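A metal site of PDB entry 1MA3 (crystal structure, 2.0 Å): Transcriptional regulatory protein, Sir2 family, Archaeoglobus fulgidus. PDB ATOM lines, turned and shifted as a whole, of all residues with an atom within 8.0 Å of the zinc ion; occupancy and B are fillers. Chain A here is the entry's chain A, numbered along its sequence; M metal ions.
The nearest printed residue that does not touch the zinc ion is Ser 155 (4.4 Å).
The backbone carbonyl oxygen of Ser 155 is in hydrogen-bond range of the backbone NH of Cys 150, 2.9 Å away. The side-chain hydroxyl (OH) of Tyr 133 lies close to the side-chain sulfur (SG) of Cys 150, at 2.9 Å. The backbone NH (N) of Ser 155 sits close to the side-chain sulfur (SG) of Cys 153, at 3.4 Å. The backbone NH (N) of Lys 152 lies close to the side-chain sulfur (SG) of Cys 150 (3.3 Å). The backbone NH (N) of Glu 131 sits close to the side-chain sulfur (SG) of Cys 129, 3.6 Å away. The backbone NH (N) of Cys 126 is in hydrogen-bond range of the backbone carbonyl oxygen (O) of Glu 131, at 2.8 Å. N of Asp 128 sits close to SG of Cys 126, 3.5 Å away.
The zinc ion is bound by the side-chain sulfur (SG) of Cys 153 (2.3 Å). SG of Cys 126 binds the zinc ion, at 2.4 Å. SG of Cys 129 binds the zinc ion, at 2.4 Å. The zinc ion is bound by the side-chain sulfur (SG) of Cys 150. The zinc ion has four donor atoms within binding distance.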
ATOM      1  N   ASP A 125       5.789   6.503  34.238  1.00  0.00           N
ATOM      2  CA  ASP A 125       4.707   6.755  33.282  1.00  0.00           C
ATOM      3  C   ASP A 125       5.226   7.516  32.061  1.00  0.00           C
ATOM      4  O   ASP A 125       6.112   8.373  32.174  1.00  0.00           O
ATOM      5  CB  ASP A 125       3.611   7.611  33.903  1.00  0.00           C
ATOM      6  CG  ASP A 125       3.006   7.000  35.148  1.00  0.00           C
ATOM      7  OD1 ASP A 125       2.127   6.122  35.037  1.00  0.00           O
ATOM      8  OD2 ASP A 125       3.396   7.411  36.254  1.00  0.00           O
ATOM      9  N   CYS A 126       4.661   7.220  30.896  1.00  0.00           N
ATOM     10  CA  CYS A 126       5.029   7.967  29.705  1.00  0.00           C
ATOM     11  C   CYS A 126       4.065   9.134  29.692  1.00  0.00           C
ATOM     12  O   CYS A 126       2.845   8.950  29.686  1.00  0.00           O
ATOM     13  CB  CYS A 126       4.815   7.140  28.437  1.00  0.00           C
ATOM     14  SG  CYS A 126       5.009   8.159  26.960  1.00  0.00           S
ATOM     15  N   LEU A 127       4.609  10.345  29.695  1.00  0.00           N
ATOM     16  CA  LEU A 127       3.770  11.543  29.700  1.00  0.00           C
ATOM     17  C   LEU A 127       2.924  11.729  28.448  1.00  0.00           C
ATOM     18  O   LEU A 127       1.861  12.342  28.495  1.00  0.00           O
ATOM     19  CB  LEU A 127       4.641  12.778  29.913  1.00  0.00           C
ATOM     20  CG  LEU A 127       4.921  13.208  31.358  1.00  0.00           C
ATOM     21  CD1 LEU A 127       4.933  12.021  32.300  1.00  0.00           C
ATOM     22  CD2 LEU A 127       6.236  13.966  31.397  1.00  0.00           C
ATOM     23  N   ASP A 128       3.407  11.206  27.317  1.00  0.00           N
ATOM     24  CA  ASP A 128       2.705  11.351  26.054  1.00  0.00           C
ATOM     25  C   ASP A 128       1.585  10.341  25.802  1.00  0.00           C
ATOM     26  O   ASP A 128       0.470  10.731  25.485  1.00  0.00           O
ATOM     27  CB  ASP A 128       3.706  11.321  24.890  1.00  0.00           C
ATOM     28  CG  ASP A 128       4.597  12.567  24.860  1.00  0.00           C
ATOM     29  OD1 ASP A 128       5.669  12.523  24.214  1.00  0.00           O
ATOM     30  OD2 ASP A 128       4.215  13.597  25.468  1.00  0.00           O
ATOM     31  N   CYS A 129       1.860   9.050  25.958  1.00  0.00           N
ATOM     32  CA  CYS A 129       0.814   8.061  25.729  1.00  0.00           C
ATOM     33  C   CYS A 129       0.251   7.459  27.023  1.00  0.00           C
ATOM     34  O   CYS A 129      -0.673   6.651  26.982  1.00  0.00           O
ATOM     35  CB  CYS A 129       1.326   6.941  24.809  1.00  0.00           C
ATOM     36  SG  CYS A 129       2.252   5.638  25.630  1.00  0.00           S
ATOM     37  N   HIS A 130       0.811   7.859  28.155  1.00  0.00           N
ATOM     38  CA  HIS A 130       0.346   7.402  29.470  1.00  0.00           C
ATOM     39  C   HIS A 130       0.651   5.954  29.855  1.00  0.00           C
ATOM     40  O   HIS A 130       0.110   5.459  30.838  1.00  0.00           O
ATOM     41  CB  HIS A 130      -1.165   7.647  29.593  1.00  0.00           C
ATOM     42  CG  HIS A 130      -1.529   9.098  29.639  1.00  0.00           C
ATOM     43  ND1 HIS A 130      -1.621   9.802  30.821  1.00  0.00           N
ATOM     44  CD2 HIS A 130      -1.755   9.992  28.642  1.00  0.00           C
ATOM     45  CE1 HIS A 130      -1.899  11.065  30.556  1.00  0.00           C
ATOM     46  NE2 HIS A 130      -1.984  11.213  29.238  1.00  0.00           N
ATOM     47  N   GLU A 131       1.494   5.272  29.088  1.00  0.00           N
ATOM     48  CA  GLU A 131       1.849   3.899  29.420  1.00  0.00           C
ATOM     49  C   GLU A 131       2.570   3.911  30.769  1.00  0.00           C
ATOM     50  O   GLU A 131       3.419   4.767  31.021  1.00  0.00           O
ATOM     51  CB  GLU A 131       2.777   3.324  28.343  1.00  0.00           C
ATOM     52  CG  GLU A 131       3.067   1.826  28.491  1.00  0.00           C
ATOM     53  CD  GLU A 131       1.880   0.968  28.103  1.00  0.00           C
ATOM     54  OE1 GLU A 131       1.897  -0.255  28.382  1.00  0.00           O
ATOM     55  OE2 GLU A 131       0.931   1.503  27.496  1.00  0.00           O
ATOM     56  N   THR A 132       2.233   2.974  31.656  1.00  0.00           N
ATOM     57  CA  THR A 132       2.894   2.901  32.957  1.00  0.00           C
ATOM     58  C   THR A 132       3.927   1.778  32.927  1.00  0.00           C
ATOM     59  O   THR A 132       3.749   0.763  32.265  1.00  0.00           O
ATOM     60  CB  THR A 132       1.901   2.621  34.102  1.00  0.00           C
ATOM     61  OG1 THR A 132       1.430   1.272  34.002  1.00  0.00           O
ATOM     62  CG2 THR A 132       0.736   3.580  34.037  1.00  0.00           C
ATOM     63  N   TYR A 133       5.021   1.970  33.665  1.00  0.00           N
ATOM     64  CA  TYR A 133       6.084   0.978  33.711  1.00  0.00           C
ATOM     65  C   TYR A 133       6.620   0.767  35.123  1.00  0.00           C
ATOM     66  O   TYR A 133       6.425   1.590  36.012  1.00  0.00           O
ATOM     67  CB  TYR A 133       7.284   1.410  32.855  1.00  0.00           C
ATOM     68  CG  TYR A 133       7.007   1.609  31.387  1.00  0.00           C
ATOM     69  CD1 TYR A 133       6.473   2.797  30.906  1.00  0.00           C
ATOM     70  CD2 TYR A 133       7.339   0.612  30.466  1.00  0.00           C
ATOM     71  CE1 TYR A 133       6.272   2.998  29.540  1.00  0.00           C
ATOM     72  CE2 TYR A 133       7.139   0.810  29.109  1.00  0.00           C
ATOM     73  CZ  TYR A 133       6.610   2.002  28.651  1.00  0.00           C
ATOM     74  OH  TYR A 133       6.453   2.190  27.304  1.00  0.00           O
ATOM     75  N   ARG A 149      13.123   5.111  27.129  1.00  0.00           N
ATOM     76  CA  ARG A 149      12.195   5.678  26.169  1.00  0.00           C
ATOM     77  C   ARG A 149      10.976   4.776  26.097  1.00  0.00           C
ATOM     78  O   ARG A 149      11.087   3.553  26.207  1.00  0.00           O
ATOM     79  CB  ARG A 149      12.871   5.783  24.796  1.00  0.00           C
ATOM     80  CG  ARG A 149      12.049   6.553  23.773  1.00  0.00           C
ATOM     81  CD  ARG A 149      12.916   7.255  22.740  1.00  0.00           C
ATOM     82  NE  ARG A 149      13.614   6.335  21.846  1.00  0.00           N
ATOM     83  CZ  ARG A 149      13.417   6.265  20.532  1.00  0.00           C
ATOM     84  NH1 ARG A 149      12.515   7.042  19.940  1.00  0.00           N
ATOM     85  NH2 ARG A 149      14.128   5.415  19.797  1.00  0.00           N
ATOM     86  N   CYS A 150       9.803   5.363  25.922  1.00  0.00           N
ATOM     87  CA  CYS A 150       8.584   4.580  25.866  1.00  0.00           C
ATOM     88  C   CYS A 150       8.627   3.534  24.748  1.00  0.00           C
ATOM     89  O   CYS A 150       8.839   3.873  23.567  1.00  0.00           O
ATOM     90  CB  CYS A 150       7.372   5.488  25.680  1.00  0.00           C
ATOM     91  SG  CYS A 150       5.839   4.557  25.743  1.00  0.00           S
ATOM     92  N   ARG A 151       8.424   2.282  25.113  1.00  0.00           N
ATOM     93  CA  ARG A 151       8.425   1.183  24.144  1.00  0.00           C
ATOM     94  C   ARG A 151       7.150   1.174  23.310  1.00  0.00           C
ATOM     95  O   ARG A 151       7.022   0.392  22.367  1.00  0.00           O
ATOM     96  CB  ARG A 151       8.570  -0.171  24.830  1.00  0.00           C
ATOM     97  CG  ARG A 151       9.970  -0.477  25.369  1.00  0.00           C
ATOM     98  CD  ARG A 151      10.052  -0.192  26.863  1.00  0.00           C
ATOM     99  NE  ARG A 151      11.265  -0.742  27.455  1.00  0.00           N
ATOM    100  CZ  ARG A 151      12.493  -0.264  27.246  1.00  0.00           C
ATOM    101  NH1 ARG A 151      13.532  -0.839  27.841  1.00  0.00           N
ATOM    102  NH2 ARG A 151      12.677   0.789  26.464  1.00  0.00           N
ATOM    103  N   LYS A 152       6.207   2.037  23.659  1.00  0.00           N
ATOM    104  CA  LYS A 152       4.943   2.121  22.950  1.00  0.00           C
ATOM    105  C   LYS A 152       4.908   3.220  21.884  1.00  0.00           C
ATOM    106  O   LYS A 152       4.611   2.953  20.711  1.00  0.00           O
ATOM    107  CB  LYS A 152       3.803   2.343  23.947  1.00  0.00           C
ATOM    108  CG  LYS A 152       2.877   1.151  24.128  1.00  0.00           C
ATOM    109  CD  LYS A 152       3.643  -0.137  24.396  1.00  0.00           C
ATOM    110  CE  LYS A 152       2.690  -1.331  24.433  1.00  0.00           C
ATOM    111  NZ  LYS A 152       3.396  -2.629  24.694  1.00  0.00           N
ATOM    112  N   CYS A 153       5.225   4.452  22.274  1.00  0.00           N
ATOM    113  CA  CYS A 153       5.192   5.572  21.335  1.00  0.00           C
ATOM    114  C   CYS A 153       6.554   6.190  21.017  1.00  0.00           C
ATOM    115  O   CYS A 153       6.644   7.093  20.201  1.00  0.00           O
ATOM    116  CB  CYS A 153       4.286   6.670  21.881  1.00  0.00           C
ATOM    117  SG  CYS A 153       5.013   7.563  23.266  1.00  0.00           S
ATOM    118  N   GLY A 154       7.610   5.719  21.687  1.00  0.00           N
ATOM    119  CA  GLY A 154       8.938   6.244  21.427  1.00  0.00           C
ATOM    120  C   GLY A 154       9.288   7.568  22.116  1.00  0.00           C
ATOM    121  O   GLY A 154      10.355   8.133  21.870  1.00  0.00           O
ATOM    122  N   SER A 155       8.408   8.052  22.973  1.00  0.00           N
ATOM    123  CA  SER A 155       8.638   9.305  23.692  1.00  0.00           C
ATOM    124  C   SER A 155       9.754   9.232  24.723  1.00  0.00           C
ATOM    125  O   SER A 155       9.950   8.196  25.380  1.00  0.00           O
ATOM    126  CB  SER A 155       7.374   9.776  24.396  1.00  0.00           C
ATOM    127  OG  SER A 155       7.644  10.923  25.192  1.00  0.00           O
ATOM    128  N   TYR A 156      10.489  10.337  24.866  1.00  0.00           N
ATOM    129  CA  TYR A 156      11.565  10.453  25.842  1.00  0.00           C
ATOM    130  C   TYR A 156      11.001  10.950  27.164  1.00  0.00           C
ATOM    131  O   TYR A 156      11.744  11.104  28.140  1.00  0.00           O
ATOM    132  CB  TYR A 156      12.616  11.457  25.364  1.00  0.00           C
ATOM    133  CG  TYR A 156      13.615  10.906  24.387  1.00  0.00           C
ATOM    134  CD1 TYR A 156      14.608  10.019  24.798  1.00  0.00           C
ATOM    135  CD2 TYR A 156      13.557  11.251  23.033  1.00  0.00           C
ATOM    136  CE1 TYR A 156      15.513   9.485  23.889  1.00  0.00           C
ATOM    137  CE2 TYR A 156      14.460  10.730  22.118  1.00  0.00           C
ATOM    138  CZ  TYR A 156      15.435   9.846  22.561  1.00  0.00           C
ATOM    139  OH  TYR A 156      16.322   9.306  21.649  1.00  0.00           O
ATOM    140  N   TYR A 157       9.700  11.220  27.200  1.00  0.00           N
ATOM    141  CA  TYR A 157       9.073  11.706  28.428  1.00  0.00           C
ATOM    142  C   TYR A 157       8.628  10.581  29.362  1.00  0.00           C
ATOM    143  O   TYR A 157       7.457  10.514  29.753  1.00  0.00           O
ATOM    144  CB  TYR A 157       7.890  12.627  28.119  1.00  0.00           C
ATOM    145  CG  TYR A 157       8.299  13.946  27.500  1.00  0.00           C
ATOM    146  CD1 TYR A 157       8.591  14.043  26.137  1.00  0.00           C
ATOM    147  CD2 TYR A 157       8.435  15.092  28.278  1.00  0.00           C
ATOM    148  CE1 TYR A 157       9.001  15.261  25.574  1.00  0.00           C
ATOM    149  CE2 TYR A 157       8.835  16.299  27.732  1.00  0.00           C
ATOM    150  CZ  TYR A 157       9.120  16.381  26.373  1.00  0.00           C
ATOM    151  OH  TYR A 157       9.537  17.570  25.831  1.00  0.00           O
ATOM    152  N   VAL A 158       9.558   9.699  29.696  1.00  0.00           N
ATOM    153  CA  VAL A 158       9.275   8.609  30.621  1.00  0.00           C
ATOM    154  C   VAL A 158       9.646   9.161  31.990  1.00  0.00           C
ATOM    155  O   VAL A 158      10.823   9.287  32.337  1.00  0.00           O
ATOM    156  CB  VAL A 158      10.114   7.368  30.284  1.00  0.00           C
ATOM    157  CG1 VAL A 158       9.876   6.276  31.318  1.00  0.00           C
ATOM    158  CG2 VAL A 158       9.754   6.864  28.892  1.00  0.00           C
HETATM  159 ZN    ZN M   1       4.471   6.578  25.302  1.00  0.00          ZN
